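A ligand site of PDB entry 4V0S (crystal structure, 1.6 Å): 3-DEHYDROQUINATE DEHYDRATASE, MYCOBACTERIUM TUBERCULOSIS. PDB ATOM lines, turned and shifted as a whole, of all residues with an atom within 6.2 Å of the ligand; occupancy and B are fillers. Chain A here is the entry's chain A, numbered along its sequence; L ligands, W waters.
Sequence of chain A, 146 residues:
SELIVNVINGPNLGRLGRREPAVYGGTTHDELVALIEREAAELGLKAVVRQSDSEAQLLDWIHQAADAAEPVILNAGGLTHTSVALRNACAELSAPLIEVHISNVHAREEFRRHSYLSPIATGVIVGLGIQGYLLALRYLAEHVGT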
ATOM      1  N   GLY A  10      32.613  11.192  -2.674  1.00  0.00           N
ATOM      2  CA  GLY A  10      31.595  10.257  -2.198  1.00  0.00           C
ATOM      3  C   GLY A  10      30.716   9.723  -3.304  1.00  0.00           C
ATOM      4  O   GLY A  10      31.058   9.756  -4.482  1.00  0.00           O
ATOM      5  N   PRO A  11      29.569   9.151  -2.914  1.00  0.00           N
ATOM      6  CA  PRO A  11      28.638   8.489  -3.854  1.00  0.00           C
ATOM      7  C   PRO A  11      28.238   9.385  -5.047  1.00  0.00           C
ATOM      8  O   PRO A  11      27.997  10.590  -4.871  1.00  0.00           O
ATOM      9  CB  PRO A  11      27.445   8.145  -2.988  1.00  0.00           C
ATOM     10  CG  PRO A  11      27.949   8.117  -1.599  1.00  0.00           C
ATOM     11  CD  PRO A  11      29.129   9.009  -1.515  1.00  0.00           C
ATOM     12  N   ASN A  12      28.198   8.760  -6.220  1.00  0.00           N
ATOM     13  CA  ASN A  12      27.823   9.354  -7.526  1.00  0.00           C
ATOM     14  C   ASN A  12      29.045   9.791  -8.297  1.00  0.00           C
ATOM     15  O   ASN A  12      29.022   9.840  -9.533  1.00  0.00           O
ATOM     16  CB  ASN A  12      26.867  10.569  -7.411  1.00  0.00           C
ATOM     17  CG  ASN A  12      25.546  10.237  -6.740  1.00  0.00           C
ATOM     18  OD1 ASN A  12      25.079   9.106  -6.766  1.00  0.00           O
ATOM     19  ND2 ASN A  12      24.935  11.229  -6.148  1.00  0.00           N
ATOM     20  N   LEU A  13      30.125  10.128  -7.586  1.00  0.00           N
ATOM     21  CA  LEU A  13      31.293  10.718  -8.255  1.00  0.00           C
ATOM     22  C   LEU A  13      32.046   9.726  -9.102  1.00  0.00           C
ATOM     23  O   LEU A  13      32.811  10.115  -9.962  1.00  0.00           O
ATOM     24  CB  LEU A  13      32.248  11.422  -7.272  1.00  0.00           C
ATOM     25  CG  LEU A  13      31.988  12.866  -6.857  1.00  0.00           C
ATOM     26  CD1 LEU A  13      32.233  13.851  -7.969  1.00  0.00           C
ATOM     27  CD2 LEU A  13      30.594  13.007  -6.334  1.00  0.00           C
ATOM     28  N   GLY A  14      31.833   8.434  -8.818  1.00  0.00           N
ATOM     29  CA  GLY A  14      32.358   7.349  -9.625  1.00  0.00           C
ATOM     30  C   GLY A  14      31.898   7.420 -11.073  1.00  0.00           C
ATOM     31  O   GLY A  14      32.611   6.975 -11.968  1.00  0.00           O
ATOM     32  N   ARG A  15      30.713   8.005 -11.291  1.00  0.00           N
ATOM     33  CA  ARG A  15      30.114   8.163 -12.615  1.00  0.00           C
ATOM     34  C   ARG A  15      30.462   9.487 -13.278  1.00  0.00           C
ATOM     35  O   ARG A  15      29.926   9.814 -14.338  1.00  0.00           O
ATOM     36  CB  ARG A  15      28.586   8.042 -12.486  1.00  0.00           C
ATOM     37  CG  ARG A  15      28.114   6.746 -11.820  1.00  0.00           C
ATOM     38  CD  ARG A  15      28.131   5.611 -12.813  1.00  0.00           C
ATOM     39  NE  ARG A  15      27.403   6.012 -14.006  1.00  0.00           N
ATOM     40  CZ  ARG A  15      27.344   5.332 -15.135  1.00  0.00           C
ATOM     41  NH1 ARG A  15      27.917   4.138 -15.281  1.00  0.00           N
ATOM     42  NH2 ARG A  15      26.664   5.865 -16.130  1.00  0.00           N
ATOM     43  N   LEU A  16      31.309  10.275 -12.642  1.00  0.00           N
ATOM     44  CA  LEU A  16      31.741  11.556 -13.198  1.00  0.00           C
ATOM     45  C   LEU A  16      32.242  11.382 -14.647  1.00  0.00           C
ATOM     46  O   LEU A  16      33.038  10.483 -14.964  1.00  0.00           O
ATOM     47  CB  LEU A  16      32.853  12.191 -12.335  1.00  0.00           C
ATOM     48  CG  LEU A  16      33.258  13.594 -12.738  1.00  0.00           C
ATOM     49  CD1 LEU A  16      32.096  14.588 -12.533  1.00  0.00           C
ATOM     50  CD2 LEU A  16      34.501  13.993 -11.955  1.00  0.00           C
ATOM     51  N   GLY A  17      31.753  12.233 -15.533  1.00  0.00           N
ATOM     52  CA  GLY A  17      32.193  12.164 -16.919  1.00  0.00           C
ATOM     53  C   GLY A  17      31.369  11.225 -17.759  1.00  0.00           C
ATOM     54  O   GLY A  17      31.342  11.367 -18.972  1.00  0.00           O
ATOM     55  N   ARG A  19      27.981   9.963 -16.467  1.00  0.00           N
ATOM     56  CA  ARG A  19      26.630  10.412 -16.211  1.00  0.00           C
ATOM     57  C   ARG A  19      26.504  11.928 -16.405  1.00  0.00           C
ATOM     58  O   ARG A  19      27.276  12.715 -15.848  1.00  0.00           O
ATOM     59  CB  ARG A  19      26.198  10.004 -14.804  1.00  0.00           C
ATOM     60  CG  ARG A  19      24.894  10.595 -14.354  1.00  0.00           C
ATOM     61  CD  ARG A  19      24.307   9.801 -13.217  1.00  0.00           C
ATOM     62  NE  ARG A  19      23.182  10.522 -12.661  1.00  0.00           N
ATOM     63  CZ  ARG A  19      22.617  10.241 -11.492  1.00  0.00           C
ATOM     64  NH1 ARG A  19      23.075   9.258 -10.719  1.00  0.00           N
ATOM     65  NH2 ARG A  19      21.597  10.960 -11.077  1.00  0.00           N
ATOM     66  N   GLU A  20      25.515  12.301 -17.216  1.00  0.00           N
ATOM     67  CA  GLU A  20      25.166  13.717 -17.426  1.00  0.00           C
ATOM     68  C   GLU A  20      26.378  14.618 -17.624  1.00  0.00           C
ATOM     69  O   GLU A  20      26.574  15.616 -16.887  1.00  0.00           O
ATOM     70  CB  GLU A  20      24.290  14.245 -16.275  1.00  0.00           C
ATOM     71  CG  GLU A  20      22.986  13.477 -16.071  1.00  0.00           C
ATOM     72  CD  GLU A  20      22.269  13.931 -14.829  1.00  0.00           C
ATOM     73  OE1 GLU A  20      21.733  15.053 -14.856  1.00  0.00           O
ATOM     74  OE2 GLU A  20      22.298  13.190 -13.820  1.00  0.00           O
ATOM     75  N   TYR A  24      27.718  17.935 -15.417  1.00  0.00           N
ATOM     76  CA  TYR A  24      28.860  17.846 -14.477  1.00  0.00           C
ATOM     77  C   TYR A  24      30.207  17.764 -15.174  1.00  0.00           C
ATOM     78  O   TYR A  24      31.275  17.668 -14.519  1.00  0.00           O
ATOM     79  CB  TYR A  24      28.699  16.659 -13.537  1.00  0.00           C
ATOM     80  CG  TYR A  24      27.366  16.638 -12.866  1.00  0.00           C
ATOM     81  CD1 TYR A  24      27.064  17.569 -11.867  1.00  0.00           C
ATOM     82  CD2 TYR A  24      26.416  15.680 -13.202  1.00  0.00           C
ATOM     83  CE1 TYR A  24      25.857  17.544 -11.228  1.00  0.00           C
ATOM     84  CE2 TYR A  24      25.170  15.677 -12.599  1.00  0.00           C
ATOM     85  CZ  TYR A  24      24.900  16.602 -11.608  1.00  0.00           C
ATOM     86  OH  TYR A  24      23.693  16.608 -10.971  1.00  0.00           O
ATOM     87  N   ASN A  75      34.205  16.157  -1.348  1.00  0.00           N
ATOM     88  CA  ASN A  75      32.973  16.291  -2.098  1.00  0.00           C
ATOM     89  C   ASN A  75      32.147  15.064  -1.752  1.00  0.00           C
ATOM     90  O   ASN A  75      32.395  13.989  -2.281  1.00  0.00           O
ATOM     91  CB  ASN A  75      33.237  16.310  -3.582  1.00  0.00           C
ATOM     92  CG  ASN A  75      31.979  16.479  -4.400  1.00  0.00           C
ATOM     93  OD1 ASN A  75      30.854  16.373  -3.896  1.00  0.00           O
ATOM     94  ND2 ASN A  75      32.168  16.770  -5.672  1.00  0.00           N
ATOM     95  N   ALA A  76      31.208  15.232  -0.820  1.00  0.00           N
ATOM     96  CA  ALA A  76      30.442  14.125  -0.291  1.00  0.00           C
ATOM     97  C   ALA A  76      29.461  13.525  -1.266  1.00  0.00           C
ATOM     98  O   ALA A  76      28.842  12.495  -0.927  1.00  0.00           O
ATOM     99  CB  ALA A  76      29.724  14.510   1.002  1.00  0.00           C
ATOM    100  N   GLY A  77      29.279  14.158  -2.428  1.00  0.00           N
ATOM    101  CA  GLY A  77      28.371  13.653  -3.428  1.00  0.00           C
ATOM    102  C   GLY A  77      26.980  13.447  -2.850  1.00  0.00           C
ATOM    103  O   GLY A  77      26.424  14.341  -2.168  1.00  0.00           O
ATOM    104  N   GLY A  78      26.431  12.235  -3.087  1.00  0.00           N
ATOM    105  CA  GLY A  78      25.099  11.895  -2.654  1.00  0.00           C
ATOM    106  C   GLY A  78      24.863  11.927  -1.137  1.00  0.00           C
ATOM    107  O   GLY A  78      23.716  11.923  -0.697  1.00  0.00           O
ATOM    108  N   LEU A  79      25.936  11.952  -0.353  1.00  0.00           N
ATOM    109  CA  LEU A  79      25.835  12.016   1.106  1.00  0.00           C
ATOM    110  C   LEU A  79      25.804  13.436   1.680  1.00  0.00           C
ATOM    111  O   LEU A  79      25.718  13.625   2.894  1.00  0.00           O
ATOM    112  CB  LEU A  79      27.008  11.250   1.722  1.00  0.00           C
ATOM    113  CG  LEU A  79      26.986   9.733   1.535  1.00  0.00           C
ATOM    114  CD1 LEU A  79      28.226   9.116   2.130  1.00  0.00           C
ATOM    115  CD2 LEU A  79      25.753   9.075   2.111  1.00  0.00           C
ATOM    116  N   THR A  80      25.913  14.431   0.815  1.00  0.00           N
ATOM    117  CA  THR A  80      26.086  15.816   1.213  1.00  0.00           C
ATOM    118  C   THR A  80      24.989  16.288   2.156  1.00  0.00           C
ATOM    119  O   THR A  80      25.300  16.931   3.169  1.00  0.00           O
ATOM    120  CB  THR A  80      26.180  16.710  -0.034  1.00  0.00           C
ATOM    121  OG1 THR A  80      27.378  16.357  -0.760  1.00  0.00           O
ATOM    122  CG2 THR A  80      26.263  18.171   0.328  1.00  0.00           C
ATOM    123  N   HIS A  81      23.735  15.963   1.819  1.00  0.00           N
ATOM    124  CA  HIS A  81      22.566  16.360   2.595  1.00  0.00           C
ATOM    125  C   HIS A  81      21.971  15.220   3.420  1.00  0.00           C
ATOM    126  O   HIS A  81      20.868  15.371   3.937  1.00  0.00           O
ATOM    127  CB  HIS A  81      21.438  16.914   1.678  1.00  0.00           C
ATOM    128  CG  HIS A  81      21.883  17.943   0.687  1.00  0.00           C
ATOM    129  ND1 HIS A  81      22.316  19.203   1.049  1.00  0.00           N
ATOM    130  CD2 HIS A  81      21.941  17.905  -0.668  1.00  0.00           C
ATOM    131  CE1 HIS A  81      22.624  19.899  -0.031  1.00  0.00           C
ATOM    132  NE2 HIS A  81      22.400  19.130  -1.090  1.00  0.00           N
ATOM    133  N   VAL A 100      33.956  20.816  -1.465  1.00  0.00           N
ATOM    134  CA  VAL A 100      33.900  21.167  -2.904  1.00  0.00           C
ATOM    135  C   VAL A 100      32.749  20.451  -3.538  1.00  0.00           C
ATOM    136  O   VAL A 100      32.554  19.271  -3.285  1.00  0.00           O
ATOM    137  CB  VAL A 100      35.194  20.786  -3.651  1.00  0.00           C
ATOM    138  CG1 VAL A 100      35.046  20.940  -5.162  1.00  0.00           C
ATOM    139  CG2 VAL A 100      36.369  21.608  -3.135  1.00  0.00           C
ATOM    140  N   HIS A 101      31.960  21.185  -4.312  1.00  0.00           N
ATOM    141  CA  HIS A 101      30.963  20.603  -5.226  1.00  0.00           C
ATOM    142  C   HIS A 101      31.174  21.129  -6.613  1.00  0.00           C
ATOM    143  O   HIS A 101      31.470  22.326  -6.788  1.00  0.00           O
ATOM    144  CB  HIS A 101      29.565  20.916  -4.735  1.00  0.00           C
ATOM    145  CG  HIS A 101      29.317  20.366  -3.361  1.00  0.00           C
ATOM    146  ND1 HIS A 101      29.149  19.028  -3.146  1.00  0.00           N
ATOM    147  CD2 HIS A 101      29.329  20.946  -2.141  1.00  0.00           C
ATOM    148  CE1 HIS A 101      28.998  18.810  -1.846  1.00  0.00           C
ATOM    149  NE2 HIS A 101      29.105  19.958  -1.213  1.00  0.00           N
ATOM    150  N   ILE A 102      31.008  20.250  -7.591  1.00  0.00           N
ATOM    151  CA  ILE A 102      31.200  20.568  -9.006  1.00  0.00           C
ATOM    152  C   ILE A 102      30.144  21.574  -9.439  1.00  0.00           C
ATOM    153  O   ILE A 102      30.436  22.591 -10.075  1.00  0.00           O
ATOM    154  CB  ILE A 102      31.205  19.262  -9.828  1.00  0.00           C
ATOM    155  CG1 ILE A 102      32.485  18.489  -9.464  1.00  0.00           C
ATOM    156  CG2 ILE A 102      31.097  19.521 -11.343  1.00  0.00           C
ATOM    157  CD1 ILE A 102      32.508  17.085  -9.984  1.00  0.00           C
ATOM    158  N   SER A 103      28.899  21.263  -9.106  1.00  0.00           N
ATOM    159  CA  SER A 103      27.736  22.068  -9.486  1.00  0.00           C
ATOM    160  C   SER A 103      27.384  22.979  -8.323  1.00  0.00           C
ATOM    161  O   SER A 103      27.821  22.764  -7.185  1.00  0.00           O
ATOM    162  CB  SER A 103      26.557  21.144  -9.791  1.00  0.00           C
ATOM    163  OG  SER A 103      26.052  20.535  -8.609  1.00  0.00           O
ATOM    164  N   ASN A 104      26.581  24.014  -8.617  1.00  0.00           N
ATOM    165  CA  ASN A 104      26.105  24.908  -7.609  1.00  0.00           C
ATOM    166  C   ASN A 104      24.882  24.310  -6.961  1.00  0.00           C
ATOM    167  O   ASN A 104      23.755  24.469  -7.420  1.00  0.00           O
ATOM    168  CB  ASN A 104      25.814  26.306  -8.164  1.00  0.00           C
ATOM    169  CG  ASN A 104      25.415  27.303  -7.065  1.00  0.00           C
ATOM    170  OD1 ASN A 104      25.231  26.909  -5.909  1.00  0.00           O
ATOM    171  ND2 ASN A 104      25.323  28.580  -7.411  1.00  0.00           N
ATOM    172  N   VAL A 105      25.137  23.607  -5.863  1.00  0.00           N
ATOM    173  CA  VAL A 105      24.111  22.913  -5.089  1.00  0.00           C
ATOM    174  C   VAL A 105      23.004  23.847  -4.619  1.00  0.00           C
ATOM    175  O   VAL A 105      21.884  23.409  -4.364  1.00  0.00           O
ATOM    176  CB  VAL A 105      24.750  22.143  -3.908  1.00  0.00           C
ATOM    177  CG1 VAL A 105      25.712  21.078  -4.441  1.00  0.00           C
ATOM    178  CG2 VAL A 105      25.415  23.092  -2.901  1.00  0.00           C
ATOM    179  N   TYR A 133      38.378  21.833  -7.275  1.00  0.00           N
ATOM    180  CA  TYR A 133      39.362  21.037  -6.558  1.00  0.00           C
ATOM    181  C   TYR A 133      40.767  21.680  -6.596  1.00  0.00           C
ATOM    182  O   TYR A 133      41.510  21.654  -5.613  1.00  0.00           O
ATOM    183  CB  TYR A 133      39.470  19.623  -7.101  1.00  0.00           C
ATOM    184  CG  TYR A 133      38.251  18.760  -6.945  1.00  0.00           C
ATOM    185  CD1 TYR A 133      38.072  17.972  -5.810  1.00  0.00           C
ATOM    186  CD2 TYR A 133      37.289  18.694  -7.924  1.00  0.00           C
ATOM    187  CE1 TYR A 133      36.976  17.145  -5.663  1.00  0.00           C
ATOM    188  CE2 TYR A 133      36.202  17.862  -7.766  1.00  0.00           C
ATOM    189  CZ  TYR A 133      36.050  17.085  -6.646  1.00  0.00           C
ATOM    190  OH  TYR A 133      34.946  16.269  -6.525  1.00  0.00           O
HETATM  191  F1  LIG L   1      29.406  15.248  -9.811  1.00  0.00           F
HETATM  192  C1  LIG L   1      28.334  14.477  -9.991  1.00  0.00           C
HETATM  193  C2  LIG L   1      28.420  13.366 -10.802  1.00  0.00           C
HETATM  194  F2  LIG L   1      29.586  13.064 -11.361  1.00  0.00           F
HETATM  195  C3  LIG L   1      27.334  12.539 -11.012  1.00  0.00           C
HETATM  196  F3  LIG L   1      27.486  11.482 -11.807  1.00  0.00           F
HETATM  197  C4  LIG L   1      26.123  12.835 -10.413  1.00  0.00           C
HETATM  198  F4  LIG L   1      25.056  12.020 -10.631  1.00  0.00           F
HETATM  199  C5  LIG L   1      26.017  13.965  -9.596  1.00  0.00           C
HETATM  200  F5  LIG L   1      24.829  14.254  -8.999  1.00  0.00           F
HETATM  201  C6  LIG L   1      27.138  14.793  -9.374  1.00  0.00           C
HETATM  202  C7  LIG L   1      27.084  16.020  -8.497  1.00  0.00           C
HETATM  203  C8  LIG L   1      27.584  15.735  -7.066  1.00  0.00           C
HETATM  204  C9  LIG L   1      27.649  17.017  -6.204  1.00  0.00           C
HETATM  205  O1  LIG L   1      28.286  16.649  -4.982  1.00  0.00           O
HETATM  206  C10 LIG L   1      28.513  18.049  -6.926  1.00  0.00           C
HETATM  207  O2  LIG L   1      29.730  17.882  -6.802  1.00  0.00           O
HETATM  208  O3  LIG L   1      27.951  18.955  -7.600  1.00  0.00           O
HETATM  209  C11 LIG L   1      26.581  14.784  -6.427  1.00  0.00           C
HETATM  210  O4  LIG L   1      26.834  13.609  -6.335  1.00  0.00           O
HETATM  211  C12 LIG L   1      25.227  15.306  -5.955  1.00  0.00           C
HETATM  212  O5  LIG L   1      24.484  14.262  -5.257  1.00  0.00           O
HETATM  213  C13 LIG L   1      25.503  16.490  -5.047  1.00  0.00           C
HETATM  214  O6  LIG L   1      24.207  17.027  -4.632  1.00  0.00           O
HETATM  215  C14 LIG L   1      26.288  17.561  -5.822  1.00  0.00           C
HETATM  216  O   HOH W   1      23.386  15.675  -2.184  1.00  0.00           O
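The backbone NH of Ser 103 lies within hydrogen-bond range of an oxygen (O3) of the ligand (2.9 Å). OG of Ser 103 sits at hydrogen-bond distance from O3 of the ligand, at 2.7 Å. OD1 of Asn 75 sits at hydrogen-bond distance from O1 of the ligand (2.8 Å). O2 of the ligand lies within hydrogen-bond range of N of Ile 102, at 2.8 Å. An oxygen (O4) of the ligand lies within hydrogen-bond range of the side-chain amide nitrogen of Asn 12. A ring nitrogen (ND1) of His 101 sits at hydrogen-bond distance from an oxygen (O1) of the ligand, at 3.1 Å.
The side-chain amide oxygen (OD1) of Asn 75 sits at hydrogen-bond distance from a ring nitrogen (ND1) of His 101. The backbone NH (N) of Gly 77 sits close to the side-chain amide oxygen (OD1) of Asn 75 (3.1 Å). OD1 of Asn 75 lies close to O of Val 100 (3.4 Å). The side-chain amide nitrogen of Asn 75 sits at hydrogen-bond distance from the side-chain hydroxyl of Tyr 133 (2.9 Å). The backbone NH of Gly 10 lies within hydrogen-bond range of the backbone carbonyl oxygen of Asn 75. NE of Arg 19 lies within salt-bridge range of OE2 of Glu 20, at 3.0 Å. O of Gly 77 is in hydrogen-bond range of OG1 of Thr 80, 2.6 Å away. N of Gly 78 is in hydrogen-bond range of O of Pro 11 (2.9 Å).
The guanidinium group (NE) of Arg 19 lies close to a fluorine (F4) of the ligand, at 3.1 Å. The side-chain hydroxyl (OH) of Tyr 24 sits close to a fluorine (F5) of the ligand. Pro 11 touches the ligand. CD1 of Leu 13 touches F1 of the ligand, at 3.7 Å. Arg 15 touches the ligand. Leu 16 touches the ligand (CD1 to F2, 3.2 Å). Gly 77 touches the ligand (CA to O4, 3.3 Å). Gly 78 touches the ligand. CG1 of Val 105 touches C14 of the ligand, at 3.8 Å. Within 4 Å of the ligand: Pro 11, Asn 12, Leu 13, Arg 15, Leu 16, Arg 19, Tyr 24, Asn 75, Gly 77, Gly 78, His 101, Ile 102, Ser 103 and Val 105.
Water W1 bridges O6 of the ligand (2.9 Å) and O of Gly 77 (3.3 Å).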
